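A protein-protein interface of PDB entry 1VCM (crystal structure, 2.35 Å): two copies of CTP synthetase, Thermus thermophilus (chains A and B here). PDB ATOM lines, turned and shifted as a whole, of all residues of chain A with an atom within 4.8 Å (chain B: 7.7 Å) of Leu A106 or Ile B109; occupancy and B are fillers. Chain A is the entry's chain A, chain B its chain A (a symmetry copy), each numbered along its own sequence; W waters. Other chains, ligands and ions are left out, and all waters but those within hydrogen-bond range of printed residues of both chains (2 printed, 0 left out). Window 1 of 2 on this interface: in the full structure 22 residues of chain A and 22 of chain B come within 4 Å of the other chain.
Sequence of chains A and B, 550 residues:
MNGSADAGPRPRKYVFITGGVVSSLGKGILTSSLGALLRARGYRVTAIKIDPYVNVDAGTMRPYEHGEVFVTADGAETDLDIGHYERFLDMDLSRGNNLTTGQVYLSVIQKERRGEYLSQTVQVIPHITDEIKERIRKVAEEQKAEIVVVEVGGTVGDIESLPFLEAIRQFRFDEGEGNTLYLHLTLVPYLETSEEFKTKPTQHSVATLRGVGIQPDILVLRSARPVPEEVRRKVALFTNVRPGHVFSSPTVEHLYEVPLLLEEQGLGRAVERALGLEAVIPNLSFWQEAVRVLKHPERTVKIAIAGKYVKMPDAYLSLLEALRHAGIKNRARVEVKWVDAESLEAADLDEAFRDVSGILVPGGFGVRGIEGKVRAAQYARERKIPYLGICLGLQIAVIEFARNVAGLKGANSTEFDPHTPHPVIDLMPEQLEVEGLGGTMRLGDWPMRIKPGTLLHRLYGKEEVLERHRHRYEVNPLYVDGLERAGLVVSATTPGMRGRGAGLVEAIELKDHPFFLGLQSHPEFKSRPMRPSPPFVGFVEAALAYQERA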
ATOM      1  N   VAL A  54      10.694 -22.883  10.479  1.00  0.00           N
ATOM      2  CA  VAL A  54      10.135 -22.389  11.726  1.00  0.00           C
ATOM      3  C   VAL A  54      11.139 -21.686  12.639  1.00  0.00           C
ATOM      4  O   VAL A  54      10.747 -20.916  13.520  1.00  0.00           O
ATOM      5  CB  VAL A  54       9.427 -23.551  12.464  1.00  0.00           C
ATOM      6  CG1 VAL A  54       8.742 -23.054  13.723  1.00  0.00           C
ATOM      7  CG2 VAL A  54       8.398 -24.191  11.527  1.00  0.00           C
ATOM      8  N   VAL A  56      13.344 -19.082  14.282  1.00  0.00           N
ATOM      9  CA  VAL A  56      13.175 -17.631  14.299  1.00  0.00           C
ATOM     10  C   VAL A  56      14.340 -16.963  13.575  1.00  0.00           C
ATOM     11  O   VAL A  56      14.175 -15.929  12.918  1.00  0.00           O
ATOM     12  CB  VAL A  56      13.070 -17.107  15.742  1.00  0.00           C
ATOM     13  CG1 VAL A  56      13.135 -15.574  15.751  1.00  0.00           C
ATOM     14  CG2 VAL A  56      11.753 -17.585  16.365  1.00  0.00           C
ATOM     15  N   THR A 101       9.274 -18.253   9.001  1.00  0.00           N
ATOM     16  CA  THR A 101       7.939 -18.599   9.478  1.00  0.00           C
ATOM     17  C   THR A 101       7.833 -18.361  10.992  1.00  0.00           C
ATOM     18  O   THR A 101       6.831 -17.839  11.484  1.00  0.00           O
ATOM     19  CB  THR A 101       7.606 -20.088   9.193  1.00  0.00           C
ATOM     20  OG1 THR A 101       7.600 -20.321   7.779  1.00  0.00           O
ATOM     21  CG2 THR A 101       6.243 -20.457   9.770  1.00  0.00           C
ATOM     22  N   GLY A 102       8.875 -18.755  11.722  1.00  0.00           N
ATOM     23  CA  GLY A 102       8.897 -18.580  13.165  1.00  0.00           C
ATOM     24  C   GLY A 102       8.732 -17.131  13.580  1.00  0.00           C
ATOM     25  O   GLY A 102       7.985 -16.829  14.513  1.00  0.00           O
ATOM     26  N   GLN A 103       9.434 -16.236  12.894  1.00  0.00           N
ATOM     27  CA  GLN A 103       9.344 -14.801  13.177  1.00  0.00           C
ATOM     28  C   GLN A 103       7.911 -14.310  12.996  1.00  0.00           C
ATOM     29  O   GLN A 103       7.314 -13.716  13.895  1.00  0.00           O
ATOM     30  CB  GLN A 103      10.244 -14.008  12.217  1.00  0.00           C
ATOM     31  CG  GLN A 103      11.731 -14.065  12.509  1.00  0.00           C
ATOM     32  CD  GLN A 103      12.561 -13.492  11.380  1.00  0.00           C
ATOM     33  OE1 GLN A 103      12.083 -12.653  10.616  1.00  0.00           O
ATOM     34  NE2 GLN A 103      13.812 -13.932  11.272  1.00  0.00           N
ATOM     35  N   VAL A 104       7.373 -14.565  11.809  1.00  0.00           N
ATOM     36  CA  VAL A 104       6.029 -14.147  11.443  1.00  0.00           C
ATOM     37  C   VAL A 104       4.931 -14.712  12.337  1.00  0.00           C
ATOM     38  O   VAL A 104       4.034 -13.984  12.768  1.00  0.00           O
ATOM     39  CB  VAL A 104       5.748 -14.516   9.963  1.00  0.00           C
ATOM     40  CG1 VAL A 104       4.295 -14.281   9.626  1.00  0.00           C
ATOM     41  CG2 VAL A 104       6.640 -13.676   9.050  1.00  0.00           C
ATOM     42  N   TYR A 105       4.984 -16.005  12.619  1.00  0.00           N
ATOM     43  CA  TYR A 105       3.959 -16.596  13.462  1.00  0.00           C
ATOM     44  C   TYR A 105       4.107 -16.175  14.928  1.00  0.00           C
ATOM     45  O   TYR A 105       3.114 -15.835  15.575  1.00  0.00           O
ATOM     46  CB  TYR A 105       3.960 -18.127  13.321  1.00  0.00           C
ATOM     47  CG  TYR A 105       3.214 -18.623  12.090  1.00  0.00           C
ATOM     48  CD1 TYR A 105       3.716 -18.415  10.804  1.00  0.00           C
ATOM     49  CD2 TYR A 105       1.998 -19.288  12.217  1.00  0.00           C
ATOM     50  CE1 TYR A 105       3.019 -18.864   9.671  1.00  0.00           C
ATOM     51  CE2 TYR A 105       1.291 -19.738  11.098  1.00  0.00           C
ATOM     52  CZ  TYR A 105       1.807 -19.526   9.831  1.00  0.00           C
ATOM     53  OH  TYR A 105       1.112 -20.003   8.745  1.00  0.00           O
ATOM     54  N   LEU A 106       5.333 -16.195  15.452  1.00  0.00           N
ATOM     55  CA  LEU A 106       5.560 -15.789  16.838  1.00  0.00           C
ATOM     56  C   LEU A 106       5.064 -14.361  17.026  1.00  0.00           C
ATOM     57  O   LEU A 106       4.311 -14.057  17.946  1.00  0.00           O
ATOM     58  CB  LEU A 106       7.054 -15.835  17.192  1.00  0.00           C
ATOM     59  CG  LEU A 106       7.399 -15.254  18.571  1.00  0.00           C
ATOM     60  CD1 LEU A 106       6.626 -16.009  19.636  1.00  0.00           C
ATOM     61  CD2 LEU A 106       8.893 -15.342  18.834  1.00  0.00           C
ATOM     62  N   SER A 107       5.490 -13.487  16.130  1.00  0.00           N
ATOM     63  CA  SER A 107       5.117 -12.083  16.188  1.00  0.00           C
ATOM     64  C   SER A 107       3.608 -11.864  16.118  1.00  0.00           C
ATOM     65  O   SER A 107       3.083 -10.958  16.761  1.00  0.00           O
ATOM     66  CB  SER A 107       5.828 -11.327  15.060  1.00  0.00           C
ATOM     67  OG  SER A 107       5.309 -10.026  14.926  1.00  0.00           O
ATOM     68  N   VAL A 108       2.908 -12.698  15.355  1.00  0.00           N
ATOM     69  CA  VAL A 108       1.461 -12.563  15.228  1.00  0.00           C
ATOM     70  C   VAL A 108       0.739 -13.158  16.421  1.00  0.00           C
ATOM     71  O   VAL A 108      -0.273 -12.620  16.874  1.00  0.00           O
ATOM     72  CB  VAL A 108       0.941 -13.226  13.931  1.00  0.00           C
ATOM     73  CG1 VAL A 108      -0.575 -13.348  13.956  1.00  0.00           C
ATOM     74  CG2 VAL A 108       1.359 -12.389  12.751  1.00  0.00           C
ATOM     75  N   ILE A 109       1.262 -14.273  16.925  1.00  0.00           N
ATOM     76  CA  ILE A 109       0.681 -14.943  18.079  1.00  0.00           C
ATOM     77  C   ILE A 109       0.821 -14.075  19.333  1.00  0.00           C
ATOM     78  O   ILE A 109      -0.094 -14.002  20.155  1.00  0.00           O
ATOM     79  CB  ILE A 109       1.365 -16.314  18.311  1.00  0.00           C
ATOM     80  CG1 ILE A 109       0.978 -17.278  17.187  1.00  0.00           C
ATOM     81  CG2 ILE A 109       0.959 -16.892  19.663  1.00  0.00           C
ATOM     82  CD1 ILE A 109       1.784 -18.570  17.189  1.00  0.00           C
ATOM     83  N   GLN A 110       1.967 -13.417  19.477  1.00  0.00           N
ATOM     84  CA  GLN A 110       2.198 -12.559  20.630  1.00  0.00           C
ATOM     85  C   GLN A 110       1.208 -11.400  20.627  1.00  0.00           C
ATOM     86  O   GLN A 110       0.692 -11.005  21.675  1.00  0.00           O
ATOM     87  CB  GLN A 110       3.646 -12.042  20.635  1.00  0.00           C
ATOM     88  CG  GLN A 110       4.665 -13.119  20.980  1.00  0.00           C
ATOM     89  CD  GLN A 110       6.103 -12.624  20.929  1.00  0.00           C
ATOM     90  OE1 GLN A 110       6.480 -11.863  20.039  1.00  0.00           O
ATOM     91  NE2 GLN A 110       6.921 -13.076  21.873  1.00  0.00           N
ATOM     92  N   VAL B  54      -5.275 -18.719  14.250  1.00  0.00           N
ATOM     93  CA  VAL B  54      -4.047 -18.436  14.975  1.00  0.00           C
ATOM     94  C   VAL B  54      -4.234 -18.188  16.471  1.00  0.00           C
ATOM     95  O   VAL B  54      -3.281 -18.305  17.246  1.00  0.00           O
ATOM     96  CB  VAL B  54      -3.318 -17.250  14.299  1.00  0.00           C
ATOM     97  CG1 VAL B  54      -1.980 -16.987  14.965  1.00  0.00           C
ATOM     98  CG2 VAL B  54      -3.110 -17.565  12.814  1.00  0.00           C
ATOM     99  N   THR B 101      -3.926 -23.432  15.519  1.00  0.00           N
ATOM    100  CA  THR B 101      -2.650 -23.156  14.865  1.00  0.00           C
ATOM    101  C   THR B 101      -1.706 -22.418  15.826  1.00  0.00           C
ATOM    102  O   THR B 101      -0.512 -22.718  15.898  1.00  0.00           O
ATOM    103  CB  THR B 101      -2.843 -22.279  13.599  1.00  0.00           C
ATOM    104  OG1 THR B 101      -3.642 -22.982  12.640  1.00  0.00           O
ATOM    105  CG2 THR B 101      -1.496 -21.929  12.974  1.00  0.00           C
ATOM    106  N   GLY B 102      -2.252 -21.447  16.556  1.00  0.00           N
ATOM    107  CA  GLY B 102      -1.463 -20.679  17.505  1.00  0.00           C
ATOM    108  C   GLY B 102      -0.802 -21.550  18.555  1.00  0.00           C
ATOM    109  O   GLY B 102       0.372 -21.356  18.880  1.00  0.00           O
ATOM    110  N   GLN B 103      -1.554 -22.504  19.092  1.00  0.00           N
ATOM    111  CA  GLN B 103      -1.027 -23.431  20.098  1.00  0.00           C
ATOM    112  C   GLN B 103       0.153 -24.216  19.534  1.00  0.00           C
ATOM    113  O   GLN B 103       1.247 -24.232  20.100  1.00  0.00           O
ATOM    114  CB  GLN B 103      -2.110 -24.436  20.519  1.00  0.00           C
ATOM    115  CG  GLN B 103      -3.184 -23.899  21.444  1.00  0.00           C
ATOM    116  CD  GLN B 103      -4.346 -24.858  21.595  1.00  0.00           C
ATOM    117  OE1 GLN B 103      -4.185 -26.066  21.422  1.00  0.00           O
ATOM    118  NE2 GLN B 103      -5.521 -24.329  21.928  1.00  0.00           N
ATOM    119  N   VAL B 104      -0.094 -24.874  18.407  1.00  0.00           N
ATOM    120  CA  VAL B 104       0.900 -25.699  17.739  1.00  0.00           C
ATOM    121  C   VAL B 104       2.158 -24.949  17.316  1.00  0.00           C
ATOM    122  O   VAL B 104       3.275 -25.420  17.537  1.00  0.00           O
ATOM    123  CB  VAL B 104       0.263 -26.399  16.510  1.00  0.00           C
ATOM    124  CG1 VAL B 104       1.323 -27.092  15.687  1.00  0.00           C
ATOM    125  CG2 VAL B 104      -0.779 -27.412  16.984  1.00  0.00           C
ATOM    126  N   TYR B 105       1.992 -23.786  16.703  1.00  0.00           N
ATOM    127  CA  TYR B 105       3.157 -23.032  16.273  1.00  0.00           C
ATOM    128  C   TYR B 105       3.907 -22.409  17.454  1.00  0.00           C
ATOM    129  O   TYR B 105       5.137 -22.473  17.508  1.00  0.00           O
ATOM    130  CB  TYR B 105       2.759 -21.964  15.241  1.00  0.00           C
ATOM    131  CG  TYR B 105       2.609 -22.511  13.829  1.00  0.00           C
ATOM    132  CD1 TYR B 105       1.555 -23.361  13.488  1.00  0.00           C
ATOM    133  CD2 TYR B 105       3.532 -22.185  12.839  1.00  0.00           C
ATOM    134  CE1 TYR B 105       1.427 -23.872  12.186  1.00  0.00           C
ATOM    135  CE2 TYR B 105       3.420 -22.689  11.541  1.00  0.00           C
ATOM    136  CZ  TYR B 105       2.366 -23.527  11.220  1.00  0.00           C
ATOM    137  OH  TYR B 105       2.255 -23.989   9.929  1.00  0.00           O
ATOM    138  N   LEU B 106       3.179 -21.810  18.397  1.00  0.00           N
ATOM    139  CA  LEU B 106       3.818 -21.208  19.566  1.00  0.00           C
ATOM    140  C   LEU B 106       4.625 -22.274  20.296  1.00  0.00           C
ATOM    141  O   LEU B 106       5.797 -22.091  20.611  1.00  0.00           O
ATOM    142  CB  LEU B 106       2.773 -20.639  20.538  1.00  0.00           C
ATOM    143  CG  LEU B 106       3.349 -20.149  21.875  1.00  0.00           C
ATOM    144  CD1 LEU B 106       4.391 -19.080  21.605  1.00  0.00           C
ATOM    145  CD2 LEU B 106       2.247 -19.604  22.769  1.00  0.00           C
ATOM    146  N   SER B 107       3.982 -23.401  20.552  1.00  0.00           N
ATOM    147  CA  SER B 107       4.614 -24.503  21.258  1.00  0.00           C
ATOM    148  C   SER B 107       5.859 -25.030  20.549  1.00  0.00           C
ATOM    149  O   SER B 107       6.822 -25.425  21.200  1.00  0.00           O
ATOM    150  CB  SER B 107       3.588 -25.625  21.460  1.00  0.00           C
ATOM    151  OG  SER B 107       4.216 -26.799  21.913  1.00  0.00           O
ATOM    152  N   VAL B 108       5.848 -25.021  19.219  1.00  0.00           N
ATOM    153  CA  VAL B 108       6.995 -25.507  18.458  1.00  0.00           C
ATOM    154  C   VAL B 108       8.098 -24.468  18.388  1.00  0.00           C
ATOM    155  O   VAL B 108       9.281 -24.806  18.442  1.00  0.00           O
ATOM    156  CB  VAL B 108       6.589 -25.921  17.025  1.00  0.00           C
ATOM    157  CG1 VAL B 108       7.818 -26.132  16.154  1.00  0.00           C
ATOM    158  CG2 VAL B 108       5.793 -27.197  17.089  1.00  0.00           C
ATOM    159  N   ILE B 109       7.703 -23.203  18.264  1.00  0.00           N
ATOM    160  CA  ILE B 109       8.654 -22.103  18.200  1.00  0.00           C
ATOM    161  C   ILE B 109       9.392 -21.951  19.534  1.00  0.00           C
ATOM    162  O   ILE B 109      10.595 -21.688  19.564  1.00  0.00           O
ATOM    163  CB  ILE B 109       7.929 -20.781  17.847  1.00  0.00           C
ATOM    164  CG1 ILE B 109       7.444 -20.832  16.397  1.00  0.00           C
ATOM    165  CG2 ILE B 109       8.861 -19.590  18.048  1.00  0.00           C
ATOM    166  CD1 ILE B 109       6.513 -19.685  16.026  1.00  0.00           C
ATOM    167  N   GLN B 110       8.668 -22.116  20.637  1.00  0.00           N
ATOM    168  CA  GLN B 110       9.275 -22.000  21.955  1.00  0.00           C
ATOM    169  C   GLN B 110      10.327 -23.085  22.145  1.00  0.00           C
ATOM    170  O   GLN B 110      11.393 -22.841  22.716  1.00  0.00           O
ATOM    171  CB  GLN B 110       8.200 -22.082  23.052  1.00  0.00           C
ATOM    172  CG  GLN B 110       7.323 -20.841  23.125  1.00  0.00           C
ATOM    173  CD  GLN B 110       6.222 -20.943  24.170  1.00  0.00           C
ATOM    174  OE1 GLN B 110       5.598 -21.991  24.333  1.00  0.00           O
ATOM    175  NE2 GLN B 110       5.961 -19.843  24.869  1.00  0.00           N
ATOM    176  N   LYS B 111      10.037 -24.277  21.633  1.00  0.00           N
ATOM    177  CA  LYS B 111      10.970 -25.389  21.747  1.00  0.00           C
ATOM    178  C   LYS B 111      12.274 -25.173  20.993  1.00  0.00           C
ATOM    179  O   LYS B 111      13.337 -25.544  21.491  1.00  0.00           O
ATOM    180  CB  LYS B 111      10.308 -26.688  21.277  1.00  0.00           C
ATOM    181  CG  LYS B 111       9.204 -27.135  22.212  1.00  0.00           C
ATOM    182  CD  LYS B 111       8.444 -28.355  21.724  1.00  0.00           C
ATOM    183  CE  LYS B 111       7.251 -28.593  22.647  1.00  0.00           C
ATOM    184  NZ  LYS B 111       6.510 -29.843  22.340  1.00  0.00           N
ATOM    185  N   GLU B 112      12.224 -24.578  19.802  1.00  0.00           N
ATOM    186  CA  GLU B 112      13.473 -24.384  19.077  1.00  0.00           C
ATOM    187  C   GLU B 112      14.261 -23.177  19.576  1.00  0.00           C
ATOM    188  O   GLU B 112      15.477 -23.154  19.436  1.00  0.00           O
ATOM    189  CB  GLU B 112      13.242 -24.327  17.556  1.00  0.00           C
ATOM    190  CG  GLU B 112      12.824 -23.011  16.973  1.00  0.00           C
ATOM    191  CD  GLU B 112      13.992 -22.093  16.666  1.00  0.00           C
ATOM    192  OE1 GLU B 112      15.033 -22.563  16.162  1.00  0.00           O
ATOM    193  OE2 GLU B 112      13.858 -20.887  16.911  1.00  0.00           O
ATOM    194  N   ARG B 113      13.593 -22.183  20.161  1.00  0.00           N
ATOM    195  CA  ARG B 113      14.335 -21.047  20.706  1.00  0.00           C
ATOM    196  C   ARG B 113      15.102 -21.548  21.933  1.00  0.00           C
ATOM    197  O   ARG B 113      16.196 -21.072  22.224  1.00  0.00           O
ATOM    198  CB  ARG B 113      13.409 -19.894  21.121  1.00  0.00           C
ATOM    199  CG  ARG B 113      12.683 -19.212  19.970  1.00  0.00           C
ATOM    200  CD  ARG B 113      13.557 -19.162  18.733  1.00  0.00           C
ATOM    201  NE  ARG B 113      14.614 -18.170  18.801  1.00  0.00           N
ATOM    202  CZ  ARG B 113      15.675 -18.153  18.000  1.00  0.00           C
ATOM    203  NH1 ARG B 113      15.837 -19.084  17.070  1.00  0.00           N
ATOM    204  NH2 ARG B 113      16.566 -17.179  18.116  1.00  0.00           N
ATOM    205  N   ARG B 114      14.520 -22.511  22.646  1.00  0.00           N
ATOM    206  CA  ARG B 114      15.169 -23.094  23.815  1.00  0.00           C
ATOM    207  C   ARG B 114      16.181 -24.142  23.367  1.00  0.00           C
ATOM    208  O   ARG B 114      16.737 -24.864  24.190  1.00  0.00           O
ATOM    209  CB  ARG B 114      14.148 -23.750  24.749  1.00  0.00           C
ATOM    210  CG  ARG B 114      13.197 -22.776  25.423  1.00  0.00           C
ATOM    211  CD  ARG B 114      12.462 -23.435  26.579  1.00  0.00           C
ATOM    212  NE  ARG B 114      11.625 -24.563  26.171  1.00  0.00           N
ATOM    213  CZ  ARG B 114      10.336 -24.463  25.856  1.00  0.00           C
ATOM    214  NH1 ARG B 114       9.734 -23.283  25.900  1.00  0.00           N
ATOM    215  NH2 ARG B 114       9.648 -25.542  25.504  1.00  0.00           N
ATOM    216  N   GLY B 115      16.405 -24.224  22.058  1.00  0.00           N
ATOM    217  CA  GLY B 115      17.364 -25.170  21.512  1.00  0.00           C
ATOM    218  C   GLY B 115      17.012 -26.641  21.637  1.00  0.00           C
ATOM    219  O   GLY B 115      17.858 -27.504  21.399  1.00  0.00           O
ATOM    220  N   TYR B 117      15.443 -28.536  19.738  1.00  0.00           N
ATOM    221  CA  TYR B 117      15.460 -29.310  18.508  1.00  0.00           C
ATOM    222  C   TYR B 117      16.888 -29.665  18.111  1.00  0.00           C
ATOM    223  O   TYR B 117      17.167 -30.030  16.967  1.00  0.00           O
ATOM    224  CB  TYR B 117      14.729 -28.571  17.390  1.00  0.00           C
ATOM    225  CG  TYR B 117      13.231 -28.732  17.512  1.00  0.00           C
ATOM    226  CD1 TYR B 117      12.412 -27.646  17.812  1.00  0.00           C
ATOM    227  CD2 TYR B 117      12.635 -29.990  17.377  1.00  0.00           C
ATOM    228  CE1 TYR B 117      11.035 -27.804  17.978  1.00  0.00           C
ATOM    229  CE2 TYR B 117      11.259 -30.159  17.545  1.00  0.00           C
ATOM    230  CZ  TYR B 117      10.468 -29.064  17.845  1.00  0.00           C
ATOM    231  OH  TYR B 117       9.115 -29.218  18.019  1.00  0.00           O
ATOM    232  N   VAL B 122      14.089 -26.405  11.764  1.00  0.00           N
ATOM    233  CA  VAL B 122      12.726 -26.824  12.067  1.00  0.00           C
ATOM    234  C   VAL B 122      11.719 -26.416  10.996  1.00  0.00           C
ATOM    235  O   VAL B 122      11.664 -25.262  10.584  1.00  0.00           O
ATOM    236  CB  VAL B 122      12.304 -26.270  13.447  1.00  0.00           C
ATOM    237  CG1 VAL B 122      11.005 -26.903  13.900  1.00  0.00           C
ATOM    238  CG2 VAL B 122      13.410 -26.548  14.465  1.00  0.00           C
ATOM    239  N   ILE B 128       6.032 -29.307  12.887  1.00  0.00           N
ATOM    240  CA  ILE B 128       4.713 -28.791  13.235  1.00  0.00           C
ATOM    241  C   ILE B 128       3.733 -29.966  13.195  1.00  0.00           C
ATOM    242  O   ILE B 128       2.898 -30.115  14.088  1.00  0.00           O
ATOM    243  CB  ILE B 128       4.258 -27.674  12.262  1.00  0.00           C
ATOM    244  CG1 ILE B 128       5.122 -26.422  12.460  1.00  0.00           C
ATOM    245  CG2 ILE B 128       2.801 -27.343  12.490  1.00  0.00           C
ATOM    246  CD1 ILE B 128       4.870 -25.686  13.761  1.00  0.00           C
ATOM    247  N   GLU B 131       4.053 -32.232  16.286  1.00  0.00           N
ATOM    248  CA  GLU B 131       3.420 -31.560  17.414  1.00  0.00           C
ATOM    249  C   GLU B 131       1.916 -31.805  17.415  1.00  0.00           C
ATOM    250  O   GLU B 131       1.329 -32.107  18.464  1.00  0.00           O
ATOM    251  CB  GLU B 131       3.704 -30.050  17.365  1.00  0.00           C
ATOM    252  CG  GLU B 131       3.018 -29.239  18.455  1.00  0.00           C
ATOM    253  CD  GLU B 131       3.596 -29.489  19.842  1.00  0.00           C
ATOM    254  OE1 GLU B 131       2.946 -29.105  20.832  1.00  0.00           O
ATOM    255  OE2 GLU B 131       4.705 -30.057  19.949  1.00  0.00           O
HETATM  256  O   HOH W   1      -0.293 -22.179   8.936  1.00  0.00           O
HETATM  257  O   HOH W   2       3.050 -22.522   7.938  1.00  0.00           O
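Ile B109 touches Val A54. Val A56 touches Ile B109 (CG2 to CG2, 3.9 Å). Arg B113 touches Val A56 (CD to CG2, 3.4 Å). Gly A102 touches Ile B109. Tyr B105 touches Tyr A105. N of Leu A106 touches CD1 of Ile B109, at 3.7 Å. Val B54 touches Ile A109. O of Gly B102 touches CD1 of Ile A109, 3.6 Å away. Leu B106 touches Ile A109 (N to CD1, 3.7 Å).
N of Val A54 is in hydrogen-bond range of O of Val B122 (2.6 Å). The side-chain carboxylate (OE2) of Glu B112 lies within hydrogen-bond range of the backbone NH (N) of Val A56 (3.2 Å).
Hydrophobic or aromatic side chains of chain B that line the printed part of chain A: Val B54, Tyr B105, Ile B109 and Val B122. Of the 12 printed residues of chain A, 6 touch a printed residue of chain B.
Printed residues of chain B within 4 Å of Tyr A105: Tyr B105 (3.3 Å). Of chain B, only Ile B109 (3.7 Å) comes within 4 Å of Leu A106. Printed residues of chain A within 4 Å of Val B54: Ile A109 (3.7 Å). Val B108 touches none of the printed residues of chain A. Of chain A, only Val A54 (3.7 Å), Val A56 (3.9 Å), Gly A102 (3.6 Å) and Leu A106 (3.7 Å) come within 4 Å of Ile B109. Printed residues of chain A within 4 Å of Glu B112: Val A56. The nearest residue of chain B that does not touch Leu A106 is Leu B106 (4.3 Å).
Val A54 touches Ile B109, and with the chains exchanged Ile A109 touches Val B54. Gly A102 touches Ile B109, and with the chains exchanged Ile A109 touches Gly B102. Tyr B105 touches its own counterpart, Tyr A105. Leu A106 touches Ile B109, and with the chains exchanged Ile A109 touches Leu B106. Positions printed for both chains: 54, 101, 102, 103, 104, 105, 106, 107, 108, 109 and 110. Of the 11 pairs that touch across the chains among the printed residues, 7 have their exchanged pair printed and touching as well.
Water W1 lies within hydrogen-bond range of the side-chain hydroxyl of Tyr A105 (2.6 Å) and the side-chain hydroxyl of Tyr B105 (3.3 Å). Water W2 bridges the side-chain hydroxyl of Tyr B105 (2.6 Å) and the side-chain hydroxyl of Tyr A105 (3.3 Å).
The backbone carbonyl oxygen (O) of Val A54 sits close to the backbone NH (N) of Gly A102 (3.4 Å). The backbone carbonyl oxygen (O) of Val A56 is in hydrogen-bond range of the side-chain amide nitrogen (NE2) of Gln A103 (2.6 Å). The backbone carbonyl oxygen (O) of Val B54 lies close to the backbone NH (N) of Gly B102, at 3.4 Å. NH1 of Arg B113 is in salt-bridge range of OE2 of Glu B112, at 2.7 Å.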
